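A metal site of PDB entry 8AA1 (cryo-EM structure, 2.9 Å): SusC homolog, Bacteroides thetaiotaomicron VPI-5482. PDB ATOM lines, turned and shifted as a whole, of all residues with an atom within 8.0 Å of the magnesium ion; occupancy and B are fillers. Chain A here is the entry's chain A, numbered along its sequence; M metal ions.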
ATOM      1  N   TYR A 832     -35.667 -14.219  -2.808  1.00  0.00           N
ATOM      2  CA  TYR A 832     -35.056 -15.522  -3.013  1.00  0.00           C
ATOM      3  C   TYR A 832     -36.084 -16.631  -2.788  1.00  0.00           C
ATOM      4  O   TYR A 832     -37.217 -16.391  -2.374  1.00  0.00           O
ATOM      5  CB  TYR A 832     -33.869 -15.714  -2.082  1.00  0.00           C
ATOM      6  CG  TYR A 832     -32.718 -14.760  -2.328  1.00  0.00           C
ATOM      7  CD1 TYR A 832     -32.774 -13.448  -1.871  1.00  0.00           C
ATOM      8  CD2 TYR A 832     -31.586 -15.172  -3.008  1.00  0.00           C
ATOM      9  CE1 TYR A 832     -31.723 -12.580  -2.090  1.00  0.00           C
ATOM     10  CE2 TYR A 832     -30.536 -14.305  -3.227  1.00  0.00           C
ATOM     11  CZ  TYR A 832     -30.609 -13.010  -2.769  1.00  0.00           C
ATOM     12  OH  TYR A 832     -29.568 -12.139  -2.998  1.00  0.00           O
ATOM     13  N   ALA A 848     -25.331 -25.752  -4.637  1.00  0.00           N
ATOM     14  CA  ALA A 848     -24.491 -24.692  -5.185  1.00  0.00           C
ATOM     15  C   ALA A 848     -23.896 -23.859  -4.064  1.00  0.00           C
ATOM     16  O   ALA A 848     -24.547 -23.613  -3.038  1.00  0.00           O
ATOM     17  CB  ALA A 848     -25.294 -23.807  -6.135  1.00  0.00           C
ATOM     18  N   THR A 849     -22.651 -23.425  -4.249  1.00  0.00           N
ATOM     19  CA  THR A 849     -21.941 -22.711  -3.199  1.00  0.00           C
ATOM     20  C   THR A 849     -22.616 -21.381  -2.880  1.00  0.00           C
ATOM     21  O   THR A 849     -23.125 -20.694  -3.775  1.00  0.00           O
ATOM     22  CB  THR A 849     -20.482 -22.493  -3.594  1.00  0.00           C
ATOM     23  OG1 THR A 849     -19.785 -21.840  -2.522  1.00  0.00           O
ATOM     24  CG2 THR A 849     -20.376 -21.655  -4.864  1.00  0.00           C
ATOM     25  N   TYR A 860     -30.928 -21.885  -0.512  1.00  0.00           N
ATOM     26  CA  TYR A 860     -31.533 -20.991  -1.492  1.00  0.00           C
ATOM     27  C   TYR A 860     -31.372 -21.577  -2.881  1.00  0.00           C
ATOM     28  O   TYR A 860     -30.280 -22.026  -3.252  1.00  0.00           O
ATOM     29  CB  TYR A 860     -30.908 -19.598  -1.422  1.00  0.00           C
ATOM     30  CG  TYR A 860     -31.232 -18.866  -0.144  1.00  0.00           C
ATOM     31  CD1 TYR A 860     -32.467 -18.267   0.051  1.00  0.00           C
ATOM     32  CD2 TYR A 860     -30.295 -18.778   0.881  1.00  0.00           C
ATOM     33  CE1 TYR A 860     -32.764 -17.596   1.216  1.00  0.00           C
ATOM     34  CE2 TYR A 860     -30.594 -18.104   2.060  1.00  0.00           C
ATOM     35  CZ  TYR A 860     -31.831 -17.517   2.213  1.00  0.00           C
ATOM     36  OH  TYR A 860     -32.118 -16.844   3.380  1.00  0.00           O
ATOM     37  N   ARG A 861     -32.465 -21.585  -3.654  1.00  0.00           N
ATOM     38  CA  ARG A 861     -32.466 -22.179  -4.976  1.00  0.00           C
ATOM     39  C   ARG A 861     -31.596 -21.387  -5.944  1.00  0.00           C
ATOM     40  O   ARG A 861     -31.539 -20.151  -5.877  1.00  0.00           O
ATOM     41  CB  ARG A 861     -33.888 -22.275  -5.506  1.00  0.00           C
ATOM     42  CG  ARG A 861     -34.036 -23.051  -6.800  1.00  0.00           C
ATOM     43  CD  ARG A 861     -35.480 -23.088  -7.253  1.00  0.00           C
ATOM     44  NE  ARG A 861     -36.364 -23.661  -6.245  1.00  0.00           N
ATOM     45  CZ  ARG A 861     -37.678 -23.746  -6.352  1.00  0.00           C
ATOM     46  NH1 ARG A 861     -38.313 -23.297  -7.431  1.00  0.00           N
ATOM     47  NH2 ARG A 861     -38.378 -24.295  -5.366  1.00  0.00           N
ATOM     48  N   ASP A 862     -30.914 -22.095  -6.834  1.00  0.00           N
ATOM     49  CA  ASP A 862     -30.093 -21.482  -7.881  1.00  0.00           C
ATOM     50  C   ASP A 862     -30.979 -21.289  -9.103  1.00  0.00           C
ATOM     51  O   ASP A 862     -31.209 -22.227  -9.873  1.00  0.00           O
ATOM     52  CB  ASP A 862     -28.878 -22.342  -8.186  1.00  0.00           C
ATOM     53  CG  ASP A 862     -27.752 -21.552  -8.810  1.00  0.00           C
ATOM     54  OD1 ASP A 862     -28.027 -20.507  -9.437  1.00  0.00           O
ATOM     55  OD2 ASP A 862     -26.578 -21.970  -8.679  1.00  0.00           O
ATOM     56  N   ILE A 863     -31.484 -20.071  -9.294  1.00  0.00           N
ATOM     57  CA  ILE A 863     -32.435 -19.811 -10.368  1.00  0.00           C
ATOM     58  C   ILE A 863     -31.769 -19.906 -11.733  1.00  0.00           C
ATOM     59  O   ILE A 863     -32.284 -20.561 -12.648  1.00  0.00           O
ATOM     60  CB  ILE A 863     -33.110 -18.446 -10.155  1.00  0.00           C
ATOM     61  CG1 ILE A 863     -33.897 -18.435  -8.843  1.00  0.00           C
ATOM     62  CG2 ILE A 863     -34.028 -18.114 -11.325  1.00  0.00           C
ATOM     63  CD1 ILE A 863     -34.664 -17.157  -8.603  1.00  0.00           C
ATOM     64  N   ASP A 864     -30.616 -19.266 -11.889  1.00  0.00           N
ATOM     65  CA  ASP A 864     -29.942 -19.234 -13.184  1.00  0.00           C
ATOM     66  C   ASP A 864     -28.984 -20.398 -13.396  1.00  0.00           C
ATOM     67  O   ASP A 864     -28.364 -20.489 -14.465  1.00  0.00           O
ATOM     68  CB  ASP A 864     -29.187 -17.899 -13.355  1.00  0.00           C
ATOM     69  CG  ASP A 864     -28.226 -17.627 -12.227  1.00  0.00           C
ATOM     70  OD1 ASP A 864     -28.166 -18.437 -11.276  1.00  0.00           O
ATOM     71  OD2 ASP A 864     -27.517 -16.597 -12.284  1.00  0.00           O
ATOM     72  N   HIS A 865     -28.836 -21.279 -12.399  1.00  0.00           N
ATOM     73  CA  HIS A 865     -28.019 -22.483 -12.516  1.00  0.00           C
ATOM     74  C   HIS A 865     -26.566 -22.149 -12.870  1.00  0.00           C
ATOM     75  O   HIS A 865     -25.930 -22.849 -13.667  1.00  0.00           O
ATOM     76  CB  HIS A 865     -28.604 -23.462 -13.533  1.00  0.00           C
ATOM     77  CG  HIS A 865     -30.003 -23.886 -13.225  1.00  0.00           C
ATOM     78  ND1 HIS A 865     -31.087 -23.047 -13.359  1.00  0.00           N
ATOM     79  CD2 HIS A 865     -30.498 -25.067 -12.783  1.00  0.00           C
ATOM     80  CE1 HIS A 865     -32.185 -23.689 -13.019  1.00  0.00           C
ATOM     81  NE2 HIS A 865     -31.858 -24.915 -12.659  1.00  0.00           N
ATOM     82  N   ASN A 866     -26.043 -21.081 -12.287  1.00  0.00           N
ATOM     83  CA  ASN A 866     -24.655 -20.703 -12.472  1.00  0.00           C
ATOM     84  C   ASN A 866     -23.729 -21.313 -11.431  1.00  0.00           C
ATOM     85  O   ASN A 866     -22.513 -21.096 -11.509  1.00  0.00           O
ATOM     86  CB  ASN A 866     -24.508 -19.172 -12.454  1.00  0.00           C
ATOM     87  CG  ASN A 866     -25.134 -18.549 -11.230  1.00  0.00           C
ATOM     88  OD1 ASN A 866     -25.618 -19.242 -10.346  1.00  0.00           O
ATOM     89  ND2 ASN A 866     -25.111 -17.223 -11.172  1.00  0.00           N
ATOM     90  N   GLY A 867     -24.264 -22.067 -10.481  1.00  0.00           N
ATOM     91  CA  GLY A 867     -23.453 -22.706  -9.464  1.00  0.00           C
ATOM     92  C   GLY A 867     -23.152 -21.865  -8.240  1.00  0.00           C
ATOM     93  O   GLY A 867     -22.517 -22.366  -7.305  1.00  0.00           O
ATOM     94  N   VAL A 868     -23.584 -20.603  -8.220  1.00  0.00           N
ATOM     95  CA  VAL A 868     -23.319 -19.702  -7.102  1.00  0.00           C
ATOM     96  C   VAL A 868     -24.592 -18.929  -6.792  1.00  0.00           C
ATOM     97  O   VAL A 868     -25.302 -18.483  -7.705  1.00  0.00           O
ATOM     98  CB  VAL A 868     -22.137 -18.759  -7.399  1.00  0.00           C
ATOM     99  CG1 VAL A 868     -22.359 -18.011  -8.702  1.00  0.00           C
ATOM    100  CG2 VAL A 868     -21.920 -17.786  -6.244  1.00  0.00           C
ATOM    101  N   ILE A 869     -24.888 -18.766  -5.506  1.00  0.00           N
ATOM    102  CA  ILE A 869     -26.047 -18.003  -5.057  1.00  0.00           C
ATOM    103  C   ILE A 869     -25.607 -16.560  -4.843  1.00  0.00           C
ATOM    104  O   ILE A 869     -24.708 -16.287  -4.049  1.00  0.00           O
ATOM    105  CB  ILE A 869     -26.651 -18.590  -3.779  1.00  0.00           C
ATOM    106  CG1 ILE A 869     -26.975 -20.072  -3.973  1.00  0.00           C
ATOM    107  CG2 ILE A 869     -27.896 -17.824  -3.378  1.00  0.00           C
ATOM    108  CD1 ILE A 869     -27.973 -20.338  -5.065  1.00  0.00           C
ATOM    109  N   ASP A 870     -26.246 -15.642  -5.560  1.00  0.00           N
ATOM    110  CA  ASP A 870     -25.914 -14.224  -5.481  1.00  0.00           C
ATOM    111  C   ASP A 870     -27.198 -13.412  -5.618  1.00  0.00           C
ATOM    112  O   ASP A 870     -28.305 -13.951  -5.540  1.00  0.00           O
ATOM    113  CB  ASP A 870     -24.872 -13.858  -6.549  1.00  0.00           C
ATOM    114  CG  ASP A 870     -25.237 -14.376  -7.929  1.00  0.00           C
ATOM    115  OD1 ASP A 870     -26.267 -15.068  -8.046  1.00  0.00           O
ATOM    116  OD2 ASP A 870     -24.497 -14.075  -8.889  1.00  0.00           O
ATOM    117  N   GLU A 871     -27.038 -12.101  -5.835  1.00  0.00           N
ATOM    118  CA  GLU A 871     -28.186 -11.216  -5.935  1.00  0.00           C
ATOM    119  C   GLU A 871     -29.021 -11.458  -7.188  1.00  0.00           C
ATOM    120  O   GLU A 871     -30.150 -10.987  -7.265  1.00  0.00           O
ATOM    121  CB  GLU A 871     -27.733  -9.762  -5.886  1.00  0.00           C
ATOM    122  CG  GLU A 871     -26.691  -9.405  -6.936  1.00  0.00           C
ATOM    123  CD  GLU A 871     -26.187  -7.981  -6.787  1.00  0.00           C
ATOM    124  OE1 GLU A 871     -26.676  -7.257  -5.900  1.00  0.00           O
ATOM    125  OE2 GLU A 871     -25.295  -7.584  -7.571  1.00  0.00           O
ATOM    126  N   ARG A 872     -28.475 -12.183  -8.176  1.00  0.00           N
ATOM    127  CA  ARG A 872     -29.223 -12.482  -9.388  1.00  0.00           C
ATOM    128  C   ARG A 872     -30.167 -13.666  -9.223  1.00  0.00           C
ATOM    129  O   ARG A 872     -30.946 -13.937 -10.135  1.00  0.00           O
ATOM    130  CB  ARG A 872     -28.259 -12.751 -10.547  1.00  0.00           C
ATOM    131  CG  ARG A 872     -27.369 -11.564 -10.896  1.00  0.00           C
ATOM    132  CD  ARG A 872     -26.647 -11.791 -12.205  1.00  0.00           C
ATOM    133  NE  ARG A 872     -25.830 -12.999 -12.186  1.00  0.00           N
ATOM    134  CZ  ARG A 872     -24.550 -13.039 -11.841  1.00  0.00           C
ATOM    135  NH1 ARG A 872     -23.902 -11.947 -11.501  1.00  0.00           N
ATOM    136  NH2 ARG A 872     -23.910 -14.204 -11.855  1.00  0.00           N
ATOM    137  N   ASP A 873     -30.099 -14.378  -8.103  1.00  0.00           N
ATOM    138  CA  ASP A 873     -30.971 -15.519  -7.853  1.00  0.00           C
ATOM    139  C   ASP A 873     -32.238 -15.091  -7.115  1.00  0.00           C
ATOM    140  O   ASP A 873     -32.564 -15.574  -6.027  1.00  0.00           O
ATOM    141  CB  ASP A 873     -30.219 -16.600  -7.082  1.00  0.00           C
ATOM    142  CG  ASP A 873     -29.311 -17.420  -7.977  1.00  0.00           C
ATOM    143  OD1 ASP A 873     -29.711 -17.713  -9.120  1.00  0.00           O
ATOM    144  OD2 ASP A 873     -28.195 -17.774  -7.539  1.00  0.00           O
ATOM    145  N   GLN A 874     -32.950 -14.148  -7.719  1.00  0.00           N
ATOM    146  CA  GLN A 874     -34.178 -13.614  -7.160  1.00  0.00           C
ATOM    147  C   GLN A 874     -35.289 -13.692  -8.201  1.00  0.00           C
ATOM    148  O   GLN A 874     -35.046 -13.621  -9.407  1.00  0.00           O
ATOM    149  CB  GLN A 874     -34.003 -12.169  -6.686  1.00  0.00           C
ATOM    150  CG  GLN A 874     -32.899 -11.978  -5.663  1.00  0.00           C
ATOM    151  CD  GLN A 874     -32.864 -10.571  -5.102  1.00  0.00           C
ATOM    152  OE1 GLN A 874     -33.889  -9.908  -5.010  1.00  0.00           O
ATOM    153  NE2 GLN A 874     -31.678 -10.119  -4.720  1.00  0.00           N
HETATM  154 MG    MG M   1     -27.106 -18.175  -9.302  1.00  0.00          MG
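The magnesium ion is bound by the side-chain amide oxygen (OD1) of Asn 866 (2.1 Å), the side-chain carboxylate (OD2) of Asp 873 (2.1 Å), the side-chain carboxylate (OD1) of Asp 864 (2.3 Å), the backbone carbonyl oxygen (O) of Val 868 (2.4 Å) and the side-chain carboxylate (OD1) of Asp 862 (2.5 Å).
The magnesium ion has five donor atoms within binding distance.
Slightly farther from the magnesium ion lies the side-chain carboxylate (OD1) of Asp 873 (2.7 Å).
OD2 of Asp 862 is in hydrogen-bond range of N of Gly 867 (2.9 Å).
N of His 865 lies close to OD1 of Asp 862.
The side-chain carboxylate (OD2) of Asp 864 is in salt-bridge range of the guanidinium group (NE) of Arg 872 (3.98 Å).
The side-chain hydroxyl (OH) of Tyr 832 sits close to the backbone carbonyl oxygen (O) of Asp 870 (3.4 Å).
ND2 of Asn 866 lies close to NH2 of Arg 872 (3.3 Å).
NH2 of Arg 872 lies within salt-bridge range of OD2 of Asp 870.
N of Ile 863 lies within hydrogen-bond range of OD1 of Asp 873 (3.0 Å).
Asp 870 touches the magnesium ion.
Six residues have an atom within 4 Å of the magnesium ion: Asp 862, Asp 864, Asn 866, Val 868, Asp 870 and Asp 873.
The nearest printed residue that does not touch the magnesium ion is Ile 869 (4.4 Å).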
